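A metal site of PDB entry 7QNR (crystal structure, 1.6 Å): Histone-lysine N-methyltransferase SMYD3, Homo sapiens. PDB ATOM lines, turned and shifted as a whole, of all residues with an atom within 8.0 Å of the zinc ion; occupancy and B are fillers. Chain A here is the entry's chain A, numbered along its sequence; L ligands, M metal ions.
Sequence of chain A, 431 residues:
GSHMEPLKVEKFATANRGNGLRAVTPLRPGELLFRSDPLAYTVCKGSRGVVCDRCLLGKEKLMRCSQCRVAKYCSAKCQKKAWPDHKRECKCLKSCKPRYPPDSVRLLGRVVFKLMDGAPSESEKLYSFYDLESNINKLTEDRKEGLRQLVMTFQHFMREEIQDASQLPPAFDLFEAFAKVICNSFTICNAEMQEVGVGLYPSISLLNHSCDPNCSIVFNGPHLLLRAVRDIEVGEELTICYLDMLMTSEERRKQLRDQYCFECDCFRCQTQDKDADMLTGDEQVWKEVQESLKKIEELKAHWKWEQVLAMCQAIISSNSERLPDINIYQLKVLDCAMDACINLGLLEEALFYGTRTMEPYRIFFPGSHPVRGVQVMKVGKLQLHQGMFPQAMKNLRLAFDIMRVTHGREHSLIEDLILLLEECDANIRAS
The zinc ion is bound by SG of Cys 264 (2.3 Å), SG of Cys 266 (2.3 Å), SG of Cys 269 (2.3 Å) and SG of Cys 211 (2.4 Å). The zinc ion has four donor atoms within binding distance.
The backbone NH of His 209 sits at hydrogen-bond distance from a nitrogen (N3) of the ligand (3.0 Å). A nitrogen (N4) of the ligand is in hydrogen-bond range of the backbone carbonyl oxygen (O) of His 209, 2.9 Å away.
SG of Cys 266 lies close to N of Arg 268 (3.6 Å). The guanidinium group of Arg 252 sits close to the side-chain sulfur of Cys 269, 3.4 Å away. The backbone NH of Cys 211 lies within hydrogen-bond range of a ring nitrogen (NE2) of His 209 (3.4 Å). SG of Cys 211 sits close to NE of Arg 252 (3.3 Å). The backbone carbonyl oxygen (O) of Cys 211 is in hydrogen-bond range of the guanidinium group (NH1) of Arg 268 (3.1 Å).
Four residues have an atom within 4 Å of the zinc ion: Cys 211, Cys 264, Cys 266 and Cys 269. The nearest printed residue that does not touch the zinc ion is His 209 (4.6 Å).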
ATOM      1  N   HIS A 209       3.994 -14.347  17.837  1.00  0.00           N
ATOM      2  CA  HIS A 209       5.048 -15.066  18.529  1.00  0.00           C
ATOM      3  C   HIS A 209       4.608 -16.477  18.899  1.00  0.00           C
ATOM      4  O   HIS A 209       3.451 -16.741  19.249  1.00  0.00           O
ATOM      5  CB  HIS A 209       5.442 -14.335  19.815  1.00  0.00           C
ATOM      6  CG  HIS A 209       6.260 -15.164  20.753  1.00  0.00           C
ATOM      7  ND1 HIS A 209       7.621 -15.276  20.630  1.00  0.00           N
ATOM      8  CD2 HIS A 209       5.906 -15.965  21.781  1.00  0.00           C
ATOM      9  CE1 HIS A 209       8.078 -16.092  21.565  1.00  0.00           C
ATOM     10  NE2 HIS A 209       7.061 -16.528  22.272  1.00  0.00           N
ATOM     11  N   SER A 210       5.576 -17.393  18.856  1.00  0.00           N
ATOM     12  CA  SER A 210       5.447 -18.699  19.466  1.00  0.00           C
ATOM     13  C   SER A 210       6.803 -19.096  20.006  1.00  0.00           C
ATOM     14  O   SER A 210       7.832 -18.829  19.373  1.00  0.00           O
ATOM     15  CB  SER A 210       4.941 -19.760  18.475  1.00  0.00           C
ATOM     16  OG  SER A 210       4.885 -21.025  19.113  1.00  0.00           O
ATOM     17  N   CYS A 211       6.820 -19.735  21.169  1.00  0.00           N
ATOM     18  CA  CYS A 211       8.058 -20.347  21.659  1.00  0.00           C
ATOM     19  C   CYS A 211       8.391 -21.641  20.918  1.00  0.00           C
ATOM     20  O   CYS A 211       9.461 -22.222  21.172  1.00  0.00           O
ATOM     21  CB  CYS A 211       7.942 -20.607  23.156  1.00  0.00           C
ATOM     22  SG  CYS A 211       7.409 -19.111  24.131  1.00  0.00           S
ATOM     23  N   ASP A 212       7.516 -22.077  20.020  1.00  0.00           N
ATOM     24  CA  ASP A 212       7.746 -23.235  19.153  1.00  0.00           C
ATOM     25  C   ASP A 212       7.286 -22.843  17.750  1.00  0.00           C
ATOM     26  O   ASP A 212       6.283 -23.347  17.239  1.00  0.00           O
ATOM     27  CB  ASP A 212       7.004 -24.462  19.677  1.00  0.00           C
ATOM     28  CG  ASP A 212       7.079 -25.652  18.728  1.00  0.00           C
ATOM     29  OD1 ASP A 212       8.075 -25.750  17.995  1.00  0.00           O
ATOM     30  OD2 ASP A 212       6.147 -26.477  18.743  1.00  0.00           O
ATOM     31  N   CYS A 241       9.695 -16.845  16.759  1.00  0.00           N
ATOM     32  CA  CYS A 241      10.006 -16.682  18.168  1.00  0.00           C
ATOM     33  C   CYS A 241      10.685 -15.329  18.359  1.00  0.00           C
ATOM     34  O   CYS A 241      11.768 -15.092  17.821  1.00  0.00           O
ATOM     35  CB  CYS A 241      10.884 -17.818  18.684  1.00  0.00           C
ATOM     36  SG  CYS A 241      11.165 -17.739  20.454  1.00  0.00           S
ATOM     37  N   LEU A 243      12.098 -14.276  20.890  1.00  0.00           N
ATOM     38  CA  LEU A 243      13.040 -14.321  21.998  1.00  0.00           C
ATOM     39  C   LEU A 243      14.181 -15.287  21.748  1.00  0.00           C
ATOM     40  O   LEU A 243      14.080 -16.222  20.952  1.00  0.00           O
ATOM     41  CB  LEU A 243      12.340 -14.753  23.291  1.00  0.00           C
ATOM     42  CG  LEU A 243      11.025 -14.064  23.647  1.00  0.00           C
ATOM     43  CD1 LEU A 243      10.336 -14.822  24.771  1.00  0.00           C
ATOM     44  CD2 LEU A 243      11.293 -12.641  24.027  1.00  0.00           C
ATOM     45  N   SER A 249      10.835 -20.654  30.909  1.00  0.00           N
ATOM     46  CA  SER A 249       9.467 -20.172  30.699  1.00  0.00           C
ATOM     47  C   SER A 249       9.186 -18.945  31.534  1.00  0.00           C
ATOM     48  O   SER A 249       8.417 -18.069  31.115  1.00  0.00           O
ATOM     49  CB  SER A 249       8.463 -21.289  31.027  1.00  0.00           C
ATOM     50  OG  SER A 249       8.490 -21.617  32.414  1.00  0.00           O
ATOM     51  N   ARG A 252      10.838 -15.962  29.762  1.00  0.00           N
ATOM     52  CA  ARG A 252      10.032 -15.626  28.594  1.00  0.00           C
ATOM     53  C   ARG A 252       8.747 -14.923  28.993  1.00  0.00           C
ATOM     54  O   ARG A 252       8.341 -13.949  28.356  1.00  0.00           O
ATOM     55  CB  ARG A 252       9.744 -16.885  27.769  1.00  0.00           C
ATOM     56  CG  ARG A 252      10.980 -17.582  27.239  1.00  0.00           C
ATOM     57  CD  ARG A 252      10.658 -18.592  26.127  1.00  0.00           C
ATOM     58  NE  ARG A 252       9.617 -19.545  26.498  1.00  0.00           N
ATOM     59  CZ  ARG A 252       9.831 -20.701  27.103  1.00  0.00           C
ATOM     60  NH1 ARG A 252      11.054 -21.095  27.448  1.00  0.00           N
ATOM     61  NH2 ARG A 252       8.795 -21.489  27.384  1.00  0.00           N
ATOM     62  N   ARG A 253       8.117 -15.380  30.077  1.00  0.00           N
ATOM     63  CA  ARG A 253       6.917 -14.714  30.592  1.00  0.00           C
ATOM     64  C   ARG A 253       7.193 -13.246  30.865  1.00  0.00           C
ATOM     65  O   ARG A 253       6.424 -12.364  30.467  1.00  0.00           O
ATOM     66  CB  ARG A 253       6.401 -15.402  31.858  1.00  0.00           C
ATOM     67  CG  ARG A 253       5.214 -14.680  32.488  1.00  0.00           C
ATOM     68  CD  ARG A 253       4.474 -15.564  33.509  1.00  0.00           C
ATOM     69  NE  ARG A 253       3.945 -16.772  32.894  1.00  0.00           N
ATOM     70  CZ  ARG A 253       4.448 -17.990  33.066  1.00  0.00           C
ATOM     71  NH1 ARG A 253       5.470 -18.202  33.880  1.00  0.00           N
ATOM     72  NH2 ARG A 253       3.902 -19.005  32.414  1.00  0.00           N
ATOM     73  N   LEU A 256       7.808 -11.258  27.513  1.00  0.00           N
ATOM     74  CA  LEU A 256       6.603 -11.128  26.690  1.00  0.00           C
ATOM     75  C   LEU A 256       5.588 -10.220  27.360  1.00  0.00           C
ATOM     76  O   LEU A 256       4.811  -9.551  26.678  1.00  0.00           O
ATOM     77  CB  LEU A 256       6.009 -12.506  26.392  1.00  0.00           C
ATOM     78  CG  LEU A 256       6.919 -13.420  25.579  1.00  0.00           C
ATOM     79  CD1 LEU A 256       6.302 -14.791  25.344  1.00  0.00           C
ATOM     80  CD2 LEU A 256       7.301 -12.775  24.244  1.00  0.00           C
ATOM     81  N   PHE A 262       1.671  -9.474  26.380  1.00  0.00           N
ATOM     82  CA  PHE A 262       0.778 -10.621  26.280  1.00  0.00           C
ATOM     83  C   PHE A 262       1.293 -11.767  27.125  1.00  0.00           C
ATOM     84  O   PHE A 262       2.481 -11.824  27.498  1.00  0.00           O
ATOM     85  CB  PHE A 262       0.551 -11.049  24.816  1.00  0.00           C
ATOM     86  CG  PHE A 262       1.727 -11.765  24.180  1.00  0.00           C
ATOM     87  CD1 PHE A 262       2.681 -11.051  23.488  1.00  0.00           C
ATOM     88  CD2 PHE A 262       1.829 -13.144  24.239  1.00  0.00           C
ATOM     89  CE1 PHE A 262       3.760 -11.696  22.902  1.00  0.00           C
ATOM     90  CE2 PHE A 262       2.904 -13.788  23.644  1.00  0.00           C
ATOM     91  CZ  PHE A 262       3.858 -13.068  22.974  1.00  0.00           C
ATOM     92  N   GLU A 263       0.358 -12.655  27.459  1.00  0.00           N
ATOM     93  CA  GLU A 263       0.603 -13.820  28.287  1.00  0.00           C
ATOM     94  C   GLU A 263       0.684 -15.001  27.337  1.00  0.00           C
ATOM     95  O   GLU A 263      -0.304 -15.326  26.668  1.00  0.00           O
ATOM     96  CB  GLU A 263      -0.535 -14.023  29.285  1.00  0.00           C
ATOM     97  CG  GLU A 263      -0.984 -12.747  30.015  1.00  0.00           C
ATOM     98  CD  GLU A 263       0.097 -12.160  30.907  1.00  0.00           C
ATOM     99  OE1 GLU A 263       1.102 -12.861  31.148  1.00  0.00           O
ATOM    100  OE2 GLU A 263      -0.065 -11.005  31.384  1.00  0.00           O
ATOM    101  N   CYS A 264       1.850 -15.621  27.243  1.00  0.00           N
ATOM    102  CA  CYS A 264       2.037 -16.696  26.268  1.00  0.00           C
ATOM    103  C   CYS A 264       1.356 -17.964  26.757  1.00  0.00           C
ATOM    104  O   CYS A 264       1.609 -18.438  27.859  1.00  0.00           O
ATOM    105  CB  CYS A 264       3.509 -16.963  26.000  1.00  0.00           C
ATOM    106  SG  CYS A 264       3.628 -18.147  24.618  1.00  0.00           S
ATOM    107  N   ASP A 265       0.498 -18.530  25.899  1.00  0.00           N
ATOM    108  CA  ASP A 265      -0.270 -19.727  26.199  1.00  0.00           C
ATOM    109  C   ASP A 265       0.230 -20.945  25.442  1.00  0.00           C
ATOM    110  O   ASP A 265      -0.446 -21.978  25.437  1.00  0.00           O
ATOM    111  CB  ASP A 265      -1.752 -19.476  25.882  1.00  0.00           C
ATOM    112  CG  ASP A 265      -2.006 -19.306  24.402  1.00  0.00           C
ATOM    113  OD1 ASP A 265      -1.031 -19.146  23.624  1.00  0.00           O
ATOM    114  OD2 ASP A 265      -3.189 -19.301  23.982  1.00  0.00           O
ATOM    115  N   CYS A 266       1.402 -20.862  24.800  1.00  0.00           N
ATOM    116  CA  CYS A 266       1.830 -21.959  23.958  1.00  0.00           C
ATOM    117  C   CYS A 266       2.104 -23.207  24.793  1.00  0.00           C
ATOM    118  O   CYS A 266       2.250 -23.153  26.024  1.00  0.00           O
ATOM    119  CB  CYS A 266       3.081 -21.590  23.160  1.00  0.00           C
ATOM    120  SG  CYS A 266       4.652 -21.617  24.063  1.00  0.00           S
ATOM    121  N   PHE A 267       2.183 -24.339  24.102  1.00  0.00           N
ATOM    122  CA  PHE A 267       2.305 -25.625  24.779  1.00  0.00           C
ATOM    123  C   PHE A 267       3.601 -25.700  25.581  1.00  0.00           C
ATOM    124  O   PHE A 267       3.638 -26.328  26.640  1.00  0.00           O
ATOM    125  CB  PHE A 267       2.235 -26.734  23.717  1.00  0.00           C
ATOM    126  CG  PHE A 267       1.990 -28.119  24.271  1.00  0.00           C
ATOM    127  CD1 PHE A 267       2.410 -29.220  23.549  1.00  0.00           C
ATOM    128  CD2 PHE A 267       1.317 -28.317  25.458  1.00  0.00           C
ATOM    129  CE1 PHE A 267       2.207 -30.501  24.028  1.00  0.00           C
ATOM    130  CE2 PHE A 267       1.093 -29.595  25.945  1.00  0.00           C
ATOM    131  CZ  PHE A 267       1.534 -30.700  25.215  1.00  0.00           C
ATOM    132  N   ARG A 268       4.665 -25.043  25.102  1.00  0.00           N
ATOM    133  CA  ARG A 268       5.927 -25.064  25.812  1.00  0.00           C
ATOM    134  C   ARG A 268       5.834 -24.316  27.143  1.00  0.00           C
ATOM    135  O   ARG A 268       6.394 -24.763  28.142  1.00  0.00           O
ATOM    136  CB  ARG A 268       7.029 -24.435  24.954  1.00  0.00           C
ATOM    137  CG  ARG A 268       7.498 -25.316  23.806  1.00  0.00           C
ATOM    138  CD  ARG A 268       8.862 -24.875  23.300  1.00  0.00           C
ATOM    139  NE  ARG A 268       9.884 -24.957  24.344  1.00  0.00           N
ATOM    140  CZ  ARG A 268      10.807 -24.039  24.583  1.00  0.00           C
ATOM    141  NH1 ARG A 268      10.902 -22.940  23.848  1.00  0.00           N
ATOM    142  NH2 ARG A 268      11.671 -24.219  25.576  1.00  0.00           N
ATOM    143  N   CYS A 269       5.147 -23.169  27.166  1.00  0.00           N
ATOM    144  CA  CYS A 269       5.027 -22.432  28.421  1.00  0.00           C
ATOM    145  C   CYS A 269       4.110 -23.145  29.398  1.00  0.00           C
ATOM    146  O   CYS A 269       4.324 -23.068  30.616  1.00  0.00           O
ATOM    147  CB  CYS A 269       4.521 -21.012  28.131  1.00  0.00           C
ATOM    148  SG  CYS A 269       5.767 -19.968  27.280  1.00  0.00           S
ATOM    149  N   GLN A 270       3.095 -23.851  28.904  1.00  0.00           N
ATOM    150  CA  GLN A 270       2.203 -24.589  29.796  1.00  0.00           C
ATOM    151  C   GLN A 270       2.919 -25.768  30.435  1.00  0.00           C
ATOM    152  O   GLN A 270       2.651 -26.094  31.602  1.00  0.00           O
ATOM    153  CB  GLN A 270       0.967 -25.081  29.031  1.00  0.00           C
ATOM    154  CG  GLN A 270       0.113 -23.993  28.440  1.00  0.00           C
ATOM    155  CD  GLN A 270      -1.188 -24.538  27.890  1.00  0.00           C
ATOM    156  OE1 GLN A 270      -1.880 -25.301  28.555  1.00  0.00           O
ATOM    157  NE2 GLN A 270      -1.535 -24.150  26.669  1.00  0.00           N
HETATM  158  N1  LIG L   1      -0.708  -9.100  16.404  1.00  0.00           N
HETATM  159  C1  LIG L   1       0.137  -8.015  15.920  1.00  0.00           C
HETATM  160  C2  LIG L   1      -0.700  -6.981  15.149  1.00  0.00           C
HETATM  161  O1  LIG L   1      -0.148  -6.060  14.554  1.00  0.00           O
HETATM  162  O2  LIG L   1      -1.937  -7.049  15.110  1.00  0.00           O
HETATM  163  C3  LIG L   1       1.263  -8.551  15.032  1.00  0.00           C
HETATM  164  C4  LIG L   1       2.487  -8.991  15.834  1.00  0.00           C
HETATM  165  S1  LIG L   1       3.320  -7.561  16.569  1.00  0.00           S
HETATM  166  C5  LIG L   1       5.034  -7.807  16.018  1.00  0.00           C
HETATM  167  C6  LIG L   1       3.528  -8.098  18.285  1.00  0.00           C
HETATM  168  C7  LIG L   1       2.266  -7.948  19.099  1.00  0.00           C
HETATM  169  O3  LIG L   1       1.280  -8.917  18.711  1.00  0.00           O
HETATM  170  C8  LIG L   1       2.498  -8.131  20.619  1.00  0.00           C
HETATM  171  O4  LIG L   1       2.830  -6.959  21.263  1.00  0.00           O
HETATM  172  C9  LIG L   1       1.138  -8.689  21.075  1.00  0.00           C
HETATM  173  O5  LIG L   1       0.268  -7.613  21.292  1.00  0.00           O
HETATM  174  C10 LIG L   1       0.674  -9.499  19.876  1.00  0.00           C
HETATM  175  N2  LIG L   1       1.091 -10.904  19.955  1.00  0.00           N
HETATM  176  C11 LIG L   1       2.179 -11.456  19.305  1.00  0.00           C
HETATM  177  N3  LIG L   1       2.241 -12.768  19.629  1.00  0.00           N
HETATM  178  C12 LIG L   1       1.215 -13.067  20.463  1.00  0.00           C
HETATM  179  C13 LIG L   1       0.811 -14.245  21.075  1.00  0.00           C
HETATM  180  N4  LIG L   1       1.475 -15.387  20.891  1.00  0.00           N
HETATM  181  N5  LIG L   1      -0.295 -14.236  21.889  1.00  0.00           N
HETATM  182  C14 LIG L   1      -0.999 -13.062  22.079  1.00  0.00           C
HETATM  183  N6  LIG L   1      -0.596 -11.907  21.477  1.00  0.00           N
HETATM  184  C15 LIG L   1       0.490 -11.889  20.661  1.00  0.00           C
HETATM  185 ZN    ZN M   1       5.252 -19.663  25.060  1.00  0.00          ZN
